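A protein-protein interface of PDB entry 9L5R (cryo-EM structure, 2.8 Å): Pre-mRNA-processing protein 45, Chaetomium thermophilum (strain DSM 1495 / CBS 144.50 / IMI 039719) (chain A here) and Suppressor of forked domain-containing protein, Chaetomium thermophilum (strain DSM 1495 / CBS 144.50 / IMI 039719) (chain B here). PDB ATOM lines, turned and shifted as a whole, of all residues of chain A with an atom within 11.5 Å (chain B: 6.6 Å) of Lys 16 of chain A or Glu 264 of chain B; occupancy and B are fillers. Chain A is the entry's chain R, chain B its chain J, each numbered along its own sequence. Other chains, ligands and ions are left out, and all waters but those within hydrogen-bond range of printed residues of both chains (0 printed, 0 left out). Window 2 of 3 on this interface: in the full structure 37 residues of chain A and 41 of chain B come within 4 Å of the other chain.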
ATOM      1  N   GLY A   7     -25.312 -21.837 -34.813  1.00  0.00           N
ATOM      2  CA  GLY A   7     -26.296 -22.757 -34.274  1.00  0.00           C
ATOM      3  C   GLY A   7     -25.770 -23.549 -33.096  1.00  0.00           C
ATOM      4  O   GLY A   7     -26.513 -23.844 -32.161  1.00  0.00           O
ATOM      5  N   LEU A   8     -24.486 -23.909 -33.127  1.00  0.00           N
ATOM      6  CA  LEU A   8     -23.877 -24.587 -31.989  1.00  0.00           C
ATOM      7  C   LEU A   8     -23.840 -23.679 -30.768  1.00  0.00           C
ATOM      8  O   LEU A   8     -24.222 -24.087 -29.662  1.00  0.00           O
ATOM      9  CB  LEU A   8     -22.471 -25.049 -32.357  1.00  0.00           C
ATOM     10  CG  LEU A   8     -21.617 -25.622 -31.234  1.00  0.00           C
ATOM     11  CD1 LEU A   8     -21.928 -27.085 -31.022  1.00  0.00           C
ATOM     12  CD2 LEU A   8     -20.157 -25.420 -31.561  1.00  0.00           C
ATOM     13  N   ALA A   9     -23.403 -22.431 -30.958  1.00  0.00           N
ATOM     14  CA  ALA A   9     -23.349 -21.491 -29.846  1.00  0.00           C
ATOM     15  C   ALA A   9     -24.738 -21.157 -29.318  1.00  0.00           C
ATOM     16  O   ALA A   9     -24.891 -20.862 -28.128  1.00  0.00           O
ATOM     17  CB  ALA A   9     -22.623 -20.218 -30.274  1.00  0.00           C
ATOM     18  N   ALA A  10     -25.754 -21.196 -30.179  1.00  0.00           N
ATOM     19  CA  ALA A  10     -27.122 -20.981 -29.726  1.00  0.00           C
ATOM     20  C   ALA A  10     -27.672 -22.195 -28.988  1.00  0.00           C
ATOM     21  O   ALA A  10     -28.355 -22.047 -27.968  1.00  0.00           O
ATOM     22  CB  ALA A  10     -28.015 -20.636 -30.915  1.00  0.00           C
ATOM     23  N   ALA A  11     -27.387 -23.400 -29.485  1.00  0.00           N
ATOM     24  CA  ALA A  11     -27.959 -24.605 -28.902  1.00  0.00           C
ATOM     25  C   ALA A  11     -27.321 -24.947 -27.568  1.00  0.00           C
ATOM     26  O   ALA A  11     -27.951 -25.609 -26.739  1.00  0.00           O
ATOM     27  CB  ALA A  11     -27.809 -25.777 -29.868  1.00  0.00           C
ATOM     28  N   LEU A  12     -26.086 -24.533 -27.346  1.00  0.00           N
ATOM     29  CA  LEU A  12     -25.433 -24.861 -26.084  1.00  0.00           C
ATOM     30  C   LEU A  12     -26.016 -24.038 -24.943  1.00  0.00           C
ATOM     31  O   LEU A  12     -26.093 -22.810 -25.047  1.00  0.00           O
ATOM     32  CB  LEU A  12     -23.932 -24.635 -26.178  1.00  0.00           C
ATOM     33  CG  LEU A  12     -23.102 -25.888 -26.416  1.00  0.00           C
ATOM     34  CD1 LEU A  12     -23.485 -26.539 -27.709  1.00  0.00           C
ATOM     35  CD2 LEU A  12     -21.648 -25.515 -26.439  1.00  0.00           C
ATOM     36  N   PRO A  13     -26.444 -24.669 -23.851  1.00  0.00           N
ATOM     37  CA  PRO A  13     -26.867 -23.909 -22.673  1.00  0.00           C
ATOM     38  C   PRO A  13     -25.686 -23.267 -21.971  1.00  0.00           C
ATOM     39  O   PRO A  13     -24.536 -23.593 -22.268  1.00  0.00           O
ATOM     40  CB  PRO A  13     -27.528 -24.970 -21.786  1.00  0.00           C
ATOM     41  CG  PRO A  13     -27.781 -26.120 -22.673  1.00  0.00           C
ATOM     42  CD  PRO A  13     -26.703 -26.105 -23.689  1.00  0.00           C
ATOM     43  N   LYS A  14     -25.951 -22.356 -21.054  1.00  0.00           N
ATOM     44  CA  LYS A  14     -24.875 -21.827 -20.240  1.00  0.00           C
ATOM     45  C   LYS A  14     -24.363 -22.907 -19.294  1.00  0.00           C
ATOM     46  O   LYS A  14     -25.133 -23.759 -18.846  1.00  0.00           O
ATOM     47  CB  LYS A  14     -25.353 -20.625 -19.437  1.00  0.00           C
ATOM     48  CG  LYS A  14     -25.560 -19.362 -20.249  1.00  0.00           C
ATOM     49  CD  LYS A  14     -24.422 -19.117 -21.228  1.00  0.00           C
ATOM     50  CE  LYS A  14     -24.888 -18.294 -22.417  1.00  0.00           C
ATOM     51  NZ  LYS A  14     -25.356 -16.944 -22.004  1.00  0.00           N
ATOM     52  N   PRO A  15     -23.065 -22.910 -18.998  1.00  0.00           N
ATOM     53  CA  PRO A  15     -22.532 -23.885 -18.039  1.00  0.00           C
ATOM     54  C   PRO A  15     -23.077 -23.626 -16.644  1.00  0.00           C
ATOM     55  O   PRO A  15     -23.044 -22.499 -16.147  1.00  0.00           O
ATOM     56  CB  PRO A  15     -21.017 -23.663 -18.107  1.00  0.00           C
ATOM     57  CG  PRO A  15     -20.849 -22.330 -18.727  1.00  0.00           C
ATOM     58  CD  PRO A  15     -21.989 -22.158 -19.661  1.00  0.00           C
ATOM     59  N   LYS A  16     -23.587 -24.683 -16.018  1.00  0.00           N
ATOM     60  CA  LYS A  16     -24.160 -24.563 -14.689  1.00  0.00           C
ATOM     61  C   LYS A  16     -23.107 -24.501 -13.598  1.00  0.00           C
ATOM     62  O   LYS A  16     -23.456 -24.257 -12.439  1.00  0.00           O
ATOM     63  CB  LYS A  16     -25.120 -25.722 -14.417  1.00  0.00           C
ATOM     64  CG  LYS A  16     -24.519 -27.094 -14.606  1.00  0.00           C
ATOM     65  CD  LYS A  16     -25.388 -28.153 -13.959  1.00  0.00           C
ATOM     66  CE  LYS A  16     -24.998 -29.548 -14.411  1.00  0.00           C
ATOM     67  NZ  LYS A  16     -25.847 -30.021 -15.533  1.00  0.00           N
ATOM     68  N   TYR A  17     -21.841 -24.719 -13.932  1.00  0.00           N
ATOM     69  CA  TYR A  17     -20.736 -24.566 -12.996  1.00  0.00           C
ATOM     70  C   TYR A  17     -19.964 -23.323 -13.411  1.00  0.00           C
ATOM     71  O   TYR A  17     -19.478 -23.239 -14.543  1.00  0.00           O
ATOM     72  CB  TYR A  17     -19.849 -25.805 -12.980  1.00  0.00           C
ATOM     73  CG  TYR A  17     -20.530 -27.010 -12.384  1.00  0.00           C
ATOM     74  CD1 TYR A  17     -21.314 -27.843 -13.164  1.00  0.00           C
ATOM     75  CD2 TYR A  17     -20.406 -27.306 -11.038  1.00  0.00           C
ATOM     76  CE1 TYR A  17     -21.943 -28.936 -12.629  1.00  0.00           C
ATOM     77  CE2 TYR A  17     -21.032 -28.404 -10.493  1.00  0.00           C
ATOM     78  CZ  TYR A  17     -21.799 -29.213 -11.295  1.00  0.00           C
ATOM     79  OH  TYR A  17     -22.430 -30.309 -10.758  1.00  0.00           O
ATOM     80  N   SER A  18     -19.877 -22.354 -12.504  1.00  0.00           N
ATOM     81  CA  SER A  18     -19.272 -21.069 -12.821  1.00  0.00           C
ATOM     82  C   SER A  18     -17.778 -21.217 -13.059  1.00  0.00           C
ATOM     83  O   SER A  18     -17.096 -21.989 -12.381  1.00  0.00           O
ATOM     84  CB  SER A  18     -19.520 -20.073 -11.693  1.00  0.00           C
ATOM     85  OG  SER A  18     -18.742 -20.396 -10.556  1.00  0.00           O
ATOM     86  N   SER A  19     -17.269 -20.464 -14.031  1.00  0.00           N
ATOM     87  CA  SER A  19     -15.861 -20.520 -14.392  1.00  0.00           C
ATOM     88  C   SER A  19     -15.203 -19.145 -14.385  1.00  0.00           C
ATOM     89  O   SER A  19     -14.017 -19.042 -14.714  1.00  0.00           O
ATOM     90  CB  SER A  19     -15.691 -21.171 -15.771  1.00  0.00           C
ATOM     91  OG  SER A  19     -16.264 -22.465 -15.804  1.00  0.00           O
ATOM     92  N   GLU A  20     -15.934 -18.091 -14.013  1.00  0.00           N
ATOM     93  CA  GLU A  20     -15.384 -16.740 -14.056  1.00  0.00           C
ATOM     94  C   GLU A  20     -14.287 -16.514 -13.022  1.00  0.00           C
ATOM     95  O   GLU A  20     -13.488 -15.586 -13.183  1.00  0.00           O
ATOM     96  CB  GLU A  20     -16.497 -15.707 -13.862  1.00  0.00           C
ATOM     97  CG  GLU A  20     -17.031 -15.618 -12.439  1.00  0.00           C
ATOM     98  CD  GLU A  20     -18.252 -16.487 -12.220  1.00  0.00           C
ATOM     99  OE1 GLU A  20     -18.630 -17.228 -13.151  1.00  0.00           O
ATOM    100  OE2 GLU A  20     -18.829 -16.438 -11.113  1.00  0.00           O
ATOM    101  N   GLU A  22     -11.950 -18.798 -12.303  1.00  0.00           N
ATOM    102  CA  GLU A  22     -10.990 -19.869 -12.532  1.00  0.00           C
ATOM    103  C   GLU A  22      -9.637 -19.290 -12.920  1.00  0.00           C
ATOM    104  O   GLU A  22      -9.532 -18.532 -13.890  1.00  0.00           O
ATOM    105  CB  GLU A  22     -11.490 -20.824 -13.615  1.00  0.00           C
ATOM    106  CG  GLU A  22     -10.705 -22.123 -13.694  1.00  0.00           C
ATOM    107  CD  GLU A  22     -11.277 -23.096 -14.701  1.00  0.00           C
ATOM    108  OE1 GLU A  22     -12.231 -22.722 -15.411  1.00  0.00           O
ATOM    109  OE2 GLU A  22     -10.770 -24.232 -14.783  1.00  0.00           O
ATOM    110  N   LYS B 261     -18.783 -32.134 -16.120  1.00  0.00           N
ATOM    111  CA  LYS B 261     -20.111 -32.428 -15.574  1.00  0.00           C
ATOM    112  C   LYS B 261     -21.191 -31.524 -16.138  1.00  0.00           C
ATOM    113  O   LYS B 261     -22.219 -31.313 -15.497  1.00  0.00           O
ATOM    114  CB  LYS B 261     -20.167 -32.387 -14.039  1.00  0.00           C
ATOM    115  CG  LYS B 261     -19.394 -33.465 -13.322  1.00  0.00           C
ATOM    116  CD  LYS B 261     -19.599 -33.309 -11.833  1.00  0.00           C
ATOM    117  CE  LYS B 261     -18.798 -34.305 -11.025  1.00  0.00           C
ATOM    118  NZ  LYS B 261     -19.281 -35.699 -11.221  1.00  0.00           N
ATOM    119  N   GLU B 262     -20.983 -30.992 -17.336  1.00  0.00           N
ATOM    120  CA  GLU B 262     -22.013 -30.245 -18.042  1.00  0.00           C
ATOM    121  C   GLU B 262     -22.745 -31.240 -18.930  1.00  0.00           C
ATOM    122  O   GLU B 262     -22.499 -31.343 -20.127  1.00  0.00           O
ATOM    123  CB  GLU B 262     -21.405 -29.118 -18.856  1.00  0.00           C
ATOM    124  CG  GLU B 262     -20.334 -28.342 -18.142  1.00  0.00           C
ATOM    125  CD  GLU B 262     -20.854 -27.570 -16.969  1.00  0.00           C
ATOM    126  OE1 GLU B 262     -22.022 -27.141 -17.003  1.00  0.00           O
ATOM    127  OE2 GLU B 262     -20.080 -27.377 -16.018  1.00  0.00           O
ATOM    128  N   TYR B 263     -23.647 -31.999 -18.315  1.00  0.00           N
ATOM    129  CA  TYR B 263     -24.333 -33.051 -19.051  1.00  0.00           C
ATOM    130  C   TYR B 263     -25.316 -32.482 -20.058  1.00  0.00           C
ATOM    131  O   TYR B 263     -25.498 -33.057 -21.134  1.00  0.00           O
ATOM    132  CB  TYR B 263     -25.027 -33.990 -18.078  1.00  0.00           C
ATOM    133  CG  TYR B 263     -24.067 -34.620 -17.111  1.00  0.00           C
ATOM    134  CD1 TYR B 263     -22.867 -35.144 -17.551  1.00  0.00           C
ATOM    135  CD2 TYR B 263     -24.345 -34.666 -15.758  1.00  0.00           C
ATOM    136  CE1 TYR B 263     -21.982 -35.706 -16.679  1.00  0.00           C
ATOM    137  CE2 TYR B 263     -23.463 -35.232 -14.877  1.00  0.00           C
ATOM    138  CZ  TYR B 263     -22.285 -35.752 -15.345  1.00  0.00           C
ATOM    139  OH  TYR B 263     -21.395 -36.321 -14.471  1.00  0.00           O
ATOM    140  N   GLU B 264     -25.930 -31.344 -19.747  1.00  0.00           N
ATOM    141  CA  GLU B 264     -26.833 -30.713 -20.700  1.00  0.00           C
ATOM    142  C   GLU B 264     -26.073 -30.155 -21.891  1.00  0.00           C
ATOM    143  O   GLU B 264     -26.521 -30.289 -23.033  1.00  0.00           O
ATOM    144  CB  GLU B 264     -27.637 -29.618 -20.008  1.00  0.00           C
ATOM    145  CG  GLU B 264     -28.790 -30.146 -19.177  1.00  0.00           C
ATOM    146  CD  GLU B 264     -28.340 -30.694 -17.839  1.00  0.00           C
ATOM    147  OE1 GLU B 264     -27.190 -30.417 -17.438  1.00  0.00           O
ATOM    148  OE2 GLU B 264     -29.130 -31.412 -17.191  1.00  0.00           O
ATOM    149  N   ARG B 265     -24.916 -29.538 -21.644  1.00  0.00           N
ATOM    150  CA  ARG B 265     -24.081 -29.046 -22.735  1.00  0.00           C
ATOM    151  C   ARG B 265     -23.544 -30.188 -23.582  1.00  0.00           C
ATOM    152  O   ARG B 265     -23.475 -30.077 -24.809  1.00  0.00           O
ATOM    153  CB  ARG B 265     -22.935 -28.210 -22.181  1.00  0.00           C
ATOM    154  CG  ARG B 265     -23.373 -26.884 -21.625  1.00  0.00           C
ATOM    155  CD  ARG B 265     -22.224 -26.144 -20.997  1.00  0.00           C
ATOM    156  NE  ARG B 265     -21.176 -25.841 -21.959  1.00  0.00           N
ATOM    157  CZ  ARG B 265     -21.152 -24.764 -22.728  1.00  0.00           C
ATOM    158  NH1 ARG B 265     -22.131 -23.881 -22.706  1.00  0.00           N
ATOM    159  NH2 ARG B 265     -20.119 -24.572 -23.539  1.00  0.00           N
ATOM    160  N   ALA B 266     -23.161 -31.293 -22.945  1.00  0.00           N
ATOM    161  CA  ALA B 266     -22.692 -32.458 -23.687  1.00  0.00           C
ATOM    162  C   ALA B 266     -23.798 -33.050 -24.549  1.00  0.00           C
ATOM    163  O   ALA B 266     -23.565 -33.409 -25.709  1.00  0.00           O
ATOM    164  CB  ALA B 266     -22.150 -33.501 -22.717  1.00  0.00           C
ATOM    165  N   ARG B 267     -25.012 -33.147 -24.000  1.00  0.00           N
ATOM    166  CA  ARG B 267     -26.146 -33.640 -24.769  1.00  0.00           C
ATOM    167  C   ARG B 267     -26.474 -32.710 -25.925  1.00  0.00           C
ATOM    168  O   ARG B 267     -26.808 -33.169 -27.021  1.00  0.00           O
ATOM    169  CB  ARG B 267     -27.354 -33.801 -23.853  1.00  0.00           C
ATOM    170  CG  ARG B 267     -28.443 -34.694 -24.391  1.00  0.00           C
ATOM    171  CD  ARG B 267     -29.467 -34.967 -23.317  1.00  0.00           C
ATOM    172  NE  ARG B 267     -29.017 -36.011 -22.406  1.00  0.00           N
ATOM    173  CZ  ARG B 267     -28.877 -35.855 -21.097  1.00  0.00           C
ATOM    174  NH1 ARG B 267     -29.159 -34.710 -20.504  1.00  0.00           N
ATOM    175  NH2 ARG B 267     -28.440 -36.875 -20.367  1.00  0.00           N
ATOM    176  N   ALA B 268     -26.373 -31.399 -25.701  1.00  0.00           N
ATOM    177  CA  ALA B 268     -26.610 -30.433 -26.768  1.00  0.00           C
ATOM    178  C   ALA B 268     -25.578 -30.557 -27.877  1.00  0.00           C
ATOM    179  O   ALA B 268     -25.925 -30.477 -29.057  1.00  0.00           O
ATOM    180  CB  ALA B 268     -26.608 -29.018 -26.198  1.00  0.00           C
ATOM    181  N   ILE B 269     -24.306 -30.761 -27.521  1.00  0.00           N
ATOM    182  CA  ILE B 269     -23.257 -30.923 -28.526  1.00  0.00           C
ATOM    183  C   ILE B 269     -23.481 -32.191 -29.338  1.00  0.00           C
ATOM    184  O   ILE B 269     -23.391 -32.177 -30.573  1.00  0.00           O
ATOM    185  CB  ILE B 269     -21.867 -30.923 -27.864  1.00  0.00           C
ATOM    186  CG1 ILE B 269     -21.513 -29.538 -27.357  1.00  0.00           C
ATOM    187  CG2 ILE B 269     -20.806 -31.344 -28.843  1.00  0.00           C
ATOM    188  CD1 ILE B 269     -20.527 -29.546 -26.249  1.00  0.00           C
ATOM    189  N   PHE B 292     -22.854 -42.258 -24.071  1.00  0.00           N
ATOM    190  CA  PHE B 292     -23.119 -41.149 -23.163  1.00  0.00           C
ATOM    191  C   PHE B 292     -24.474 -41.288 -22.493  1.00  0.00           C
ATOM    192  O   PHE B 292     -24.604 -41.055 -21.288  1.00  0.00           O
ATOM    193  CB  PHE B 292     -23.054 -39.826 -23.915  1.00  0.00           C
ATOM    194  CG  PHE B 292     -23.658 -38.681 -23.160  1.00  0.00           C
ATOM    195  CD1 PHE B 292     -23.017 -38.161 -22.055  1.00  0.00           C
ATOM    196  CD2 PHE B 292     -24.866 -38.134 -23.542  1.00  0.00           C
ATOM    197  CE1 PHE B 292     -23.561 -37.121 -21.353  1.00  0.00           C
ATOM    198  CE2 PHE B 292     -25.413 -37.095 -22.835  1.00  0.00           C
ATOM    199  CZ  PHE B 292     -24.757 -36.588 -21.742  1.00  0.00           C
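O of Pro 13 of chain A sits at hydrogen-bond distance from NH1 of Arg 265 of chain B, 2.5 Å away.
The side-chain carboxylate (OE2) of Glu 264 of chain B is in salt-bridge range of the side-chain amino group (NZ) of Lys 16 of chain A (3.9 Å).
OE1 of Glu 262 of chain B sits at hydrogen-bond distance from N of Lys 16 of chain A.
Ala 11 of chain A touches Ala 268 of chain B.
Leu 12 of chain A touches Arg 265 of chain B (CD2 to NH2, 3.4 Å).
CD1 of Leu 12 of chain A touches CG1 of Ile 269 of chain B, at 3.6 Å.
Ala 268 of chain B touches Pro 13 of chain A.
Pro 15 of chain A touches Glu 262 of chain B.
CD of Pro 15 of chain A touches NH1 of Arg 265 of chain B, 3.5 Å away.
Lys 16 of chain A touches Lys 261 of chain B (CE to O, 3.5 Å).
Lys 261 of chain B touches Tyr 17 of chain A (O to CE1, 3.7 Å).
Tyr 17 of chain A touches Glu 262 of chain B (CD1 to OE2, 3.1 Å).
Of chain B, only Lys 261 (3.5 Å), Glu 262 (3.1 Å) and Glu 264 (2.4 Å) come within 4 Å of Lys 16 of chain A.
Glu 264 of chain B touches just one residue of chain A: Lys 16 (2.4 Å).
No residue of chain A comes within 4 Å of Ala 266 of chain B.
Ala 268 of chain B touches two residues of chain A.
Of the printed residues of chain A, Arg 265 of chain B touches Leu 12 (3.4 Å), Pro 13 (2.5 Å) and Pro 15 (3.5 Å).
Printed residues of chain B within 4 Å of Pro 15 of chain A: Glu 262 (3.5 Å) and Arg 265 (3.5 Å).
Printed residues of chain A within 4 Å of Lys 261 of chain B: Lys 16 and Tyr 17.
Of the printed residues of chain A, Ile 269 of chain B touches Leu 12 (3.6 Å).
Lys 14 of chain A touches none of the printed residues of chain B.
Leu 8 of chain A touches none of the printed residues of chain B.
Hydrophobic or aromatic side chains of chain A within 4 Å of the printed part of chain B: Leu 12, Pro 13, Pro 15 and Tyr 17.
Printed residues of chain B that touch a printed residue of chain A: Lys 261, Glu 262, Glu 264, Arg 265, Ala 268 and Ile 269.
Hydrophobic or aromatic side chains of chain B within 4 Å of the printed part of chain A: Ala 268 and Ile 269.
Among the printed residues, 12 pairs touch across the chains.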
